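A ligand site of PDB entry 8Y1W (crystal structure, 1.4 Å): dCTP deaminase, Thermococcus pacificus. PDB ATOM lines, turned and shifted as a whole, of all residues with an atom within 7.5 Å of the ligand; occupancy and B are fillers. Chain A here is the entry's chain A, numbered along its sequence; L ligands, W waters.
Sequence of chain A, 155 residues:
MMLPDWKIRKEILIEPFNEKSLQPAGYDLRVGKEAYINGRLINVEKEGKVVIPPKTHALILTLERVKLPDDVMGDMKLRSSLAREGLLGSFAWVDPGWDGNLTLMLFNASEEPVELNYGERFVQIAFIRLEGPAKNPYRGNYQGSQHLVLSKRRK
The backbone NH of Ala 92 is in hydrogen-bond range of an oxygen (O2) of the ligand (3.2 Å).
An oxygen (O3) of the ligand sits at hydrogen-bond distance from the backbone NH (N) of Asp 95, 3.0 Å away.
An oxygen (O1) of the ligand lies within hydrogen-bond range of the backbone NH (N) of Thr 103, at 3.1 Å.
O3 of the ligand is in hydrogen-bond range of OD2 of Asp 95, at 2.7 Å.
A nitrogen (N2) of the ligand lies within hydrogen-bond range of the backbone carbonyl oxygen (O) of Thr 103 (2.9 Å).
The side-chain hydroxyl (OG1) of Thr 103 is in hydrogen-bond range of the backbone NH (N) of Val 149 (3.0 Å).
N of Gly 74 lies within hydrogen-bond range of O of Val 94 (2.9 Å).
O of Leu 104 sits at hydrogen-bond distance from N of Ile 60 (2.8 Å).
O of Trp 98 is in hydrogen-bond range of N of Leu 68, at 2.8 Å.
N of Tyr 138 sits at hydrogen-bond distance from O of Pro 96.
O of Gly 100 lies within hydrogen-bond range of NE1 of Trp 98 (3.0 Å).
Met 76 touches the ligand (CE to O2, 3.5 Å).
CA of Phe 91 touches O2 of the ligand, 3.7 Å away.
O of Trp 93 touches C4 of the ligand (3.3 Å).
Val 94 touches the ligand (CG1 to C6, 3.9 Å).
Trp 98 touches the ligand (CD2 to C6, 3.5 Å).
Leu 102 touches the ligand (CD2 to N1, 3.4 Å).
Leu 104 touches the ligand.
CE2 of Tyr 138 touches O7 of the ligand, 3.1 Å away.
Hydrophobic or aromatic side chains that line the ligand: Met 76, Ala 92, Val 94, Trp 98, Leu 102, Leu 104 and Tyr 138.
Within 4 Å of the ligand: Met 76, Phe 91, Ala 92, Trp 93, Val 94, Asp 95, Trp 98, Leu 102, Thr 103, Leu 104 and Tyr 138.
The nearest printed residue that does not touch the ligand is Ser 90 (4.4 Å).
Water W3 lies within hydrogen-bond range of the backbone carbonyl oxygen (O) of Ser 90 (2.7 Å), an oxygen (O2) of the ligand (2.8 Å) and the backbone NH (N) of Met 105 (3.0 Å).
Water W1 lies within hydrogen-bond range of O of Thr 103 (3.0 Å) and O1 of the ligand (3.3 Å).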
ATOM      1  N   ILE A  60     -17.859  20.159   1.769  1.00  0.00           N
ATOM      2  CA  ILE A  60     -17.386  19.466   0.570  1.00  0.00           C
ATOM      3  C   ILE A  60     -16.410  18.394   1.014  1.00  0.00           C
ATOM      4  O   ILE A  60     -15.475  18.695   1.773  1.00  0.00           O
ATOM      5  CB  ILE A  60     -16.701  20.446  -0.419  1.00  0.00           C
ATOM      6  CG1 ILE A  60     -17.708  21.543  -0.878  1.00  0.00           C
ATOM      7  CG2 ILE A  60     -16.146  19.642  -1.602  1.00  0.00           C
ATOM      8  CD1 ILE A  60     -17.121  22.586  -1.790  1.00  0.00           C
ATOM      9  N   LEU A  61     -16.572  17.176   0.493  1.00  0.00           N
ATOM     10  CA  LEU A  61     -15.655  16.081   0.794  1.00  0.00           C
ATOM     11  C   LEU A  61     -14.482  16.123  -0.177  1.00  0.00           C
ATOM     12  O   LEU A  61     -14.688  16.315  -1.376  1.00  0.00           O
ATOM     13  CB  LEU A  61     -16.415  14.763   0.589  1.00  0.00           C
ATOM     14  CG  LEU A  61     -15.668  13.483   1.032  1.00  0.00           C
ATOM     15  CD1 LEU A  61     -15.397  13.521   2.558  1.00  0.00           C
ATOM     16  CD2 LEU A  61     -16.495  12.277   0.680  1.00  0.00           C
ATOM     17  N   LEU A  68      -1.721  10.994   7.628  1.00  0.00           N
ATOM     18  CA  LEU A  68      -0.577  11.692   8.210  1.00  0.00           C
ATOM     19  C   LEU A  68       0.173  10.802   9.193  1.00  0.00           C
ATOM     20  O   LEU A  68      -0.448  10.186  10.060  1.00  0.00           O
ATOM     21  CB  LEU A  68      -1.071  12.934   8.936  1.00  0.00           C
ATOM     22  CG  LEU A  68      -1.297  14.138   8.020  1.00  0.00           C
ATOM     23  CD1 LEU A  68      -2.464  13.954   7.126  1.00  0.00           C
ATOM     24  CD2 LEU A  68      -1.514  15.328   8.912  1.00  0.00           C
ATOM     25  N   MET A  73       1.795  17.499  11.012  1.00  0.00           N
ATOM     26  CA  MET A  73       0.501  18.202  11.137  1.00  0.00           C
ATOM     27  C   MET A  73       0.114  18.774   9.756  1.00  0.00           C
ATOM     28  O   MET A  73       0.997  19.292   9.087  1.00  0.00           O
ATOM     29  CB  MET A  73       0.677  19.354  12.131  1.00  0.00           C
ATOM     30  CG  MET A  73      -0.535  20.272  12.232  1.00  0.00           C
ATOM     31  SD  MET A  73      -1.827  19.664  13.348  1.00  0.00           S
ATOM     32  CE  MET A  73      -1.622  20.782  14.740  1.00  0.00           C
ATOM     33  N   GLY A  74      -1.164  18.669   9.374  1.00  0.00           N
ATOM     34  CA  GLY A  74      -1.622  19.222   8.097  1.00  0.00           C
ATOM     35  C   GLY A  74      -2.302  20.574   8.251  1.00  0.00           C
ATOM     36  O   GLY A  74      -3.112  20.792   9.159  1.00  0.00           O
ATOM     37  N   MET A  76      -4.276  23.588   5.987  1.00  0.00           N
ATOM     38  CA  MET A  76      -4.958  23.850   4.731  1.00  0.00           C
ATOM     39  C   MET A  76      -5.277  25.314   4.511  1.00  0.00           C
ATOM     40  O   MET A  76      -5.621  26.038   5.455  1.00  0.00           O
ATOM     41  CB  MET A  76      -6.276  23.086   4.730  1.00  0.00           C
ATOM     42  CG  MET A  76      -6.074  21.566   4.809  1.00  0.00           C
ATOM     43  SD  MET A  76      -7.588  20.634   4.666  1.00  0.00           S
ATOM     44  CE  MET A  76      -8.284  20.941   6.309  1.00  0.00           C
ATOM     45  N   SER A  90     -13.225  27.495   6.163  1.00  0.00           N
ATOM     46  CA  SER A  90     -13.164  27.443   7.614  1.00  0.00           C
ATOM     47  C   SER A  90     -12.581  26.108   7.989  1.00  0.00           C
ATOM     48  O   SER A  90     -13.306  25.131   8.055  1.00  0.00           O
ATOM     49  CB  SER A  90     -14.560  27.636   8.197  1.00  0.00           C
ATOM     50  OG  SER A  90     -14.398  27.699   9.596  1.00  0.00           O
ATOM     51  N   PHE A  91     -11.282  26.071   8.191  1.00  0.00           N
ATOM     52  CA  PHE A  91     -10.565  24.823   8.288  1.00  0.00           C
ATOM     53  C   PHE A  91     -10.015  24.570   9.679  1.00  0.00           C
ATOM     54  O   PHE A  91      -9.527  25.496  10.337  1.00  0.00           O
ATOM     55  CB  PHE A  91      -9.421  24.730   7.292  1.00  0.00           C
ATOM     56  CG  PHE A  91      -9.855  24.888   5.835  1.00  0.00           C
ATOM     57  CD1 PHE A  91     -11.020  24.334   5.328  1.00  0.00           C
ATOM     58  CD2 PHE A  91      -9.080  25.640   5.035  1.00  0.00           C
ATOM     59  CE1 PHE A  91     -11.380  24.584   3.974  1.00  0.00           C
ATOM     60  CE2 PHE A  91      -9.467  25.887   3.694  1.00  0.00           C
ATOM     61  CZ  PHE A  91     -10.556  25.358   3.189  1.00  0.00           C
ATOM     62  N   ALA A  92     -10.061  23.319  10.137  1.00  0.00           N
ATOM     63  CA  ALA A  92      -9.429  22.881  11.389  1.00  0.00           C
ATOM     64  C   ALA A  92      -8.053  22.342  11.078  1.00  0.00           C
ATOM     65  O   ALA A  92      -7.732  22.052   9.935  1.00  0.00           O
ATOM     66  CB  ALA A  92     -10.267  21.780  12.055  1.00  0.00           C
ATOM     67  N   TRP A  93      -7.244  22.179  12.119  1.00  0.00           N
ATOM     68  CA  TRP A  93      -5.975  21.466  11.934  1.00  0.00           C
ATOM     69  C   TRP A  93      -6.243  20.014  11.512  1.00  0.00           C
ATOM     70  O   TRP A  93      -7.263  19.435  11.848  1.00  0.00           O
ATOM     71  CB  TRP A  93      -5.212  21.432  13.261  1.00  0.00           C
ATOM     72  CG  TRP A  93      -4.646  22.747  13.605  1.00  0.00           C
ATOM     73  CD1 TRP A  93      -5.026  23.569  14.605  1.00  0.00           C
ATOM     74  CD2 TRP A  93      -3.525  23.377  12.968  1.00  0.00           C
ATOM     75  NE1 TRP A  93      -4.205  24.686  14.633  1.00  0.00           N
ATOM     76  CE2 TRP A  93      -3.264  24.588  13.648  1.00  0.00           C
ATOM     77  CE3 TRP A  93      -2.705  23.003  11.907  1.00  0.00           C
ATOM     78  CZ2 TRP A  93      -2.240  25.472  13.259  1.00  0.00           C
ATOM     79  CZ3 TRP A  93      -1.646  23.870  11.535  1.00  0.00           C
ATOM     80  CH2 TRP A  93      -1.418  25.067  12.237  1.00  0.00           C
ATOM     81  N   VAL A  94      -5.335  19.442  10.706  1.00  0.00           N
ATOM     82  CA  VAL A  94      -5.383  18.007  10.382  1.00  0.00           C
ATOM     83  C   VAL A  94      -4.347  17.314  11.274  1.00  0.00           C
ATOM     84  O   VAL A  94      -3.137  17.509  11.122  1.00  0.00           O
ATOM     85  CB  VAL A  94      -5.095  17.765   8.884  1.00  0.00           C
ATOM     86  CG1 VAL A  94      -5.275  16.280   8.562  1.00  0.00           C
ATOM     87  CG2 VAL A  94      -6.002  18.614   8.003  1.00  0.00           C
ATOM     88  N   ASP A  95      -4.846  16.609  12.284  1.00  0.00           N
ATOM     89  CA  ASP A  95      -4.005  16.151  13.377  1.00  0.00           C
ATOM     90  C   ASP A  95      -3.042  15.038  12.951  1.00  0.00           C
ATOM     91  O   ASP A  95      -3.360  14.230  12.070  1.00  0.00           O
ATOM     92  CB  ASP A  95      -4.879  15.671  14.541  1.00  0.00           C
ATOM     93  CG  ASP A  95      -5.762  16.786  15.071  1.00  0.00           C
ATOM     94  OD1 ASP A  95      -5.227  17.733  15.701  1.00  0.00           O
ATOM     95  OD2 ASP A  95      -7.002  16.757  14.823  1.00  0.00           O
ATOM     96  N   PRO A  96      -1.855  14.997  13.551  1.00  0.00           N
ATOM     97  CA  PRO A  96      -0.946  13.864  13.357  1.00  0.00           C
ATOM     98  C   PRO A  96      -1.697  12.570  13.615  1.00  0.00           C
ATOM     99  O   PRO A  96      -2.384  12.440  14.611  1.00  0.00           O
ATOM    100  CB  PRO A  96       0.136  14.083  14.433  1.00  0.00           C
ATOM    101  CG  PRO A  96       0.191  15.602  14.614  1.00  0.00           C
ATOM    102  CD  PRO A  96      -1.306  15.974  14.510  1.00  0.00           C
ATOM    103  N   GLY A  97      -1.548  11.621  12.686  1.00  0.00           N
ATOM    104  CA  GLY A  97      -2.241  10.334  12.771  1.00  0.00           C
ATOM    105  C   GLY A  97      -3.563  10.303  12.035  1.00  0.00           C
ATOM    106  O   GLY A  97      -4.135   9.221  11.876  1.00  0.00           O
ATOM    107  N   TRP A  98      -4.077  11.447  11.570  1.00  0.00           N
ATOM    108  CA  TRP A  98      -5.307  11.434  10.796  1.00  0.00           C
ATOM    109  C   TRP A  98      -5.192  10.492   9.600  1.00  0.00           C
ATOM    110  O   TRP A  98      -4.177  10.466   8.903  1.00  0.00           O
ATOM    111  CB  TRP A  98      -5.602  12.846  10.285  1.00  0.00           C
ATOM    112  CG  TRP A  98      -6.694  12.830   9.244  1.00  0.00           C
ATOM    113  CD1 TRP A  98      -6.557  12.920   7.877  1.00  0.00           C
ATOM    114  CD2 TRP A  98      -8.087  12.660   9.489  1.00  0.00           C
ATOM    115  NE1 TRP A  98      -7.778  12.846   7.264  1.00  0.00           N
ATOM    116  CE2 TRP A  98      -8.737  12.658   8.238  1.00  0.00           C
ATOM    117  CE3 TRP A  98      -8.841  12.443  10.645  1.00  0.00           C
ATOM    118  CZ2 TRP A  98     -10.128  12.536   8.116  1.00  0.00           C
ATOM    119  CZ3 TRP A  98     -10.229  12.276  10.529  1.00  0.00           C
ATOM    120  CH2 TRP A  98     -10.855  12.323   9.259  1.00  0.00           C
ATOM    121  N   ASP A  99      -6.269   9.794   9.294  1.00  0.00           N
ATOM    122  CA  ASP A  99      -6.341   8.978   8.089  1.00  0.00           C
ATOM    123  C   ASP A  99      -7.762   9.085   7.533  1.00  0.00           C
ATOM    124  O   ASP A  99      -8.668   8.496   8.115  1.00  0.00           O
ATOM    125  CB  ASP A  99      -5.980   7.522   8.445  1.00  0.00           C
ATOM    126  CG  ASP A  99      -5.918   6.634   7.243  1.00  0.00           C
ATOM    127  OD1 ASP A  99      -6.275   7.058   6.130  1.00  0.00           O
ATOM    128  OD2 ASP A  99      -5.472   5.474   7.399  1.00  0.00           O
ATOM    129  N   GLY A 100      -7.974   9.751   6.416  1.00  0.00           N
ATOM    130  CA  GLY A 100      -9.290   9.758   5.789  1.00  0.00           C
ATOM    131  C   GLY A 100      -9.468  10.869   4.769  1.00  0.00           C
ATOM    132  O   GLY A 100      -8.624  11.769   4.608  1.00  0.00           O
ATOM    133  N   ASN A 101     -10.605  10.833   4.088  1.00  0.00           N
ATOM    134  CA  ASN A 101     -11.045  12.009   3.313  1.00  0.00           C
ATOM    135  C   ASN A 101     -11.535  13.094   4.248  1.00  0.00           C
ATOM    136  O   ASN A 101     -12.118  12.784   5.288  1.00  0.00           O
ATOM    137  CB  ASN A 101     -12.218  11.591   2.397  1.00  0.00           C
ATOM    138  CG  ASN A 101     -11.829  10.525   1.398  1.00  0.00           C
ATOM    139  OD1 ASN A 101     -11.548   9.397   1.787  1.00  0.00           O
ATOM    140  ND2 ASN A 101     -11.810  10.871   0.108  1.00  0.00           N
ATOM    141  N   LEU A 102     -11.300  14.340   3.888  1.00  0.00           N
ATOM    142  CA  LEU A 102     -11.575  15.467   4.767  1.00  0.00           C
ATOM    143  C   LEU A 102     -12.913  16.108   4.416  1.00  0.00           C
ATOM    144  O   LEU A 102     -13.236  16.286   3.227  1.00  0.00           O
ATOM    145  CB  LEU A 102     -10.433  16.504   4.666  1.00  0.00           C
ATOM    146  CG  LEU A 102      -9.092  16.000   5.181  1.00  0.00           C
ATOM    147  CD1 LEU A 102      -7.925  16.728   4.517  1.00  0.00           C
ATOM    148  CD2 LEU A 102      -9.064  16.079   6.684  1.00  0.00           C
ATOM    149  N   THR A 103     -13.675  16.500   5.442  1.00  0.00           N
ATOM    150  CA  THR A 103     -14.901  17.271   5.249  1.00  0.00           C
ATOM    151  C   THR A 103     -14.547  18.734   5.477  1.00  0.00           C
ATOM    152  O   THR A 103     -14.186  19.146   6.596  1.00  0.00           O
ATOM    153  CB  THR A 103     -15.956  16.808   6.246  1.00  0.00           C
ATOM    154  OG1 THR A 103     -16.335  15.451   5.975  1.00  0.00           O
ATOM    155  CG2 THR A 103     -17.200  17.655   6.132  1.00  0.00           C
ATOM    156  N   LEU A 104     -14.659  19.519   4.441  1.00  0.00           N
ATOM    157  CA  LEU A 104     -14.200  20.911   4.425  1.00  0.00           C
ATOM    158  C   LEU A 104     -15.377  21.887   4.303  1.00  0.00           C
ATOM    159  O   LEU A 104     -16.209  21.766   3.396  1.00  0.00           O
ATOM    160  CB  LEU A 104     -13.216  21.137   3.286  1.00  0.00           C
ATOM    161  CG  LEU A 104     -11.976  20.243   3.320  1.00  0.00           C
ATOM    162  CD1 LEU A 104     -11.004  20.670   2.277  1.00  0.00           C
ATOM    163  CD2 LEU A 104     -11.314  20.233   4.708  1.00  0.00           C
ATOM    164  N   MET A 105     -15.389  22.930   5.122  1.00  0.00           N
ATOM    165  CA  MET A 105     -16.451  23.917   5.051  1.00  0.00           C
ATOM    166  C   MET A 105     -15.931  25.128   4.279  1.00  0.00           C
ATOM    167  O   MET A 105     -14.820  25.649   4.539  1.00  0.00           O
ATOM    168  CB  MET A 105     -16.910  24.318   6.464  1.00  0.00           C
ATOM    169  CG  MET A 105     -17.996  25.370   6.489  1.00  0.00           C
ATOM    170  SD  MET A 105     -17.603  27.073   6.062  1.00  0.00           S
ATOM    171  CE  MET A 105     -18.165  27.930   7.509  1.00  0.00           C
ATOM    172  N   TYR A 138      -3.698  11.086  16.860  1.00  0.00           N
ATOM    173  CA  TYR A 138      -5.103  10.901  16.561  1.00  0.00           C
ATOM    174  C   TYR A 138      -5.233   9.457  16.070  1.00  0.00           C
ATOM    175  O   TYR A 138      -5.967   8.643  16.643  1.00  0.00           O
ATOM    176  CB  TYR A 138      -5.499  11.872  15.458  1.00  0.00           C
ATOM    177  CG  TYR A 138      -6.951  11.845  15.064  1.00  0.00           C
ATOM    178  CD1 TYR A 138      -7.454  10.871  14.210  1.00  0.00           C
ATOM    179  CD2 TYR A 138      -7.815  12.871  15.473  1.00  0.00           C
ATOM    180  CE1 TYR A 138      -8.787  10.850  13.835  1.00  0.00           C
ATOM    181  CE2 TYR A 138      -9.166  12.881  15.088  1.00  0.00           C
ATOM    182  CZ  TYR A 138      -9.637  11.866  14.267  1.00  0.00           C
ATOM    183  OH  TYR A 138     -10.966  11.854  13.895  1.00  0.00           O
ATOM    184  N   VAL A 149     -18.770  14.056   7.048  1.00  0.00           N
ATOM    185  CA  VAL A 149     -19.184  14.029   8.448  1.00  0.00           C
ATOM    186  C   VAL A 149     -20.303  15.040   8.615  1.00  0.00           C
ATOM    187  O   VAL A 149     -20.132  16.241   8.368  1.00  0.00           O
ATOM    188  CB  VAL A 149     -18.033  14.374   9.380  1.00  0.00           C
ATOM    189  CG1 VAL A 149     -18.518  14.478  10.800  1.00  0.00           C
ATOM    190  CG2 VAL A 149     -16.950  13.308   9.228  1.00  0.00           C
ATOM    191  N   SER A 151     -22.462  15.101  11.494  1.00  0.00           N
ATOM    192  CA  SER A 151     -22.906  15.254  12.869  1.00  0.00           C
ATOM    193  C   SER A 151     -22.732  16.719  13.291  1.00  0.00           C
ATOM    194  O   SER A 151     -21.974  17.499  12.687  1.00  0.00           O
ATOM    195  CB  SER A 151     -22.036  14.373  13.758  1.00  0.00           C
ATOM    196  OG  SER A 151     -20.708  14.844  13.588  1.00  0.00           O
HETATM  197  N1  LIG L   1     -10.457  17.530   9.437  1.00  0.00           N
HETATM  198  C1  LIG L   1     -11.543  17.698   8.588  1.00  0.00           C
HETATM  199  N2  LIG L   1     -11.748  18.985   8.145  1.00  0.00           N
HETATM  200  C2  LIG L   1     -10.983  20.102   8.460  1.00  0.00           C
HETATM  201  C3  LIG L   1      -9.871  19.844   9.324  1.00  0.00           C
HETATM  202  C4  LIG L   1      -9.672  18.608   9.793  1.00  0.00           C
HETATM  203  O1  LIG L   1     -12.257  16.766   8.237  1.00  0.00           O
HETATM  204  O2  LIG L   1     -11.320  21.207   8.022  1.00  0.00           O
HETATM  205  C5  LIG L   1     -10.202  16.215  10.023  1.00  0.00           C
HETATM  206  C6  LIG L   1      -8.732  15.942  10.362  1.00  0.00           C
HETATM  207  C7  LIG L   1      -8.659  16.250  11.843  1.00  0.00           C
HETATM  208  C8  LIG L   1     -10.028  15.800  12.328  1.00  0.00           C
HETATM  209  O3  LIG L   1      -7.612  15.536  12.518  1.00  0.00           O
HETATM  210  O4  LIG L   1     -10.917  16.152  11.251  1.00  0.00           O
HETATM  211  C9  LIG L   1     -10.489  16.434  13.626  1.00  0.00           C
HETATM  212  O5  LIG L   1     -11.769  15.879  13.995  1.00  0.00           O
HETATM  213  P1  LIG L   1     -12.228  15.798  15.511  1.00  0.00           P
HETATM  214  O6  LIG L   1     -13.776  15.397  15.491  1.00  0.00           O
HETATM  215  O7  LIG L   1     -11.179  14.889  16.327  1.00  0.00           O
HETATM  216  O8  LIG L   1     -12.106  17.316  16.031  1.00  0.00           O
HETATM  217  O   HOH W   1     -14.921  18.344   9.362  1.00  0.00           O
HETATM  218  O   HOH W   2     -13.838  14.629   9.216  1.00  0.00           O
HETATM  219  O   HOH W   3     -13.768  22.497   7.585  1.00  0.00           O
HETATM  220  O   HOH W   4     -13.641  16.426  11.142  1.00  0.00           O
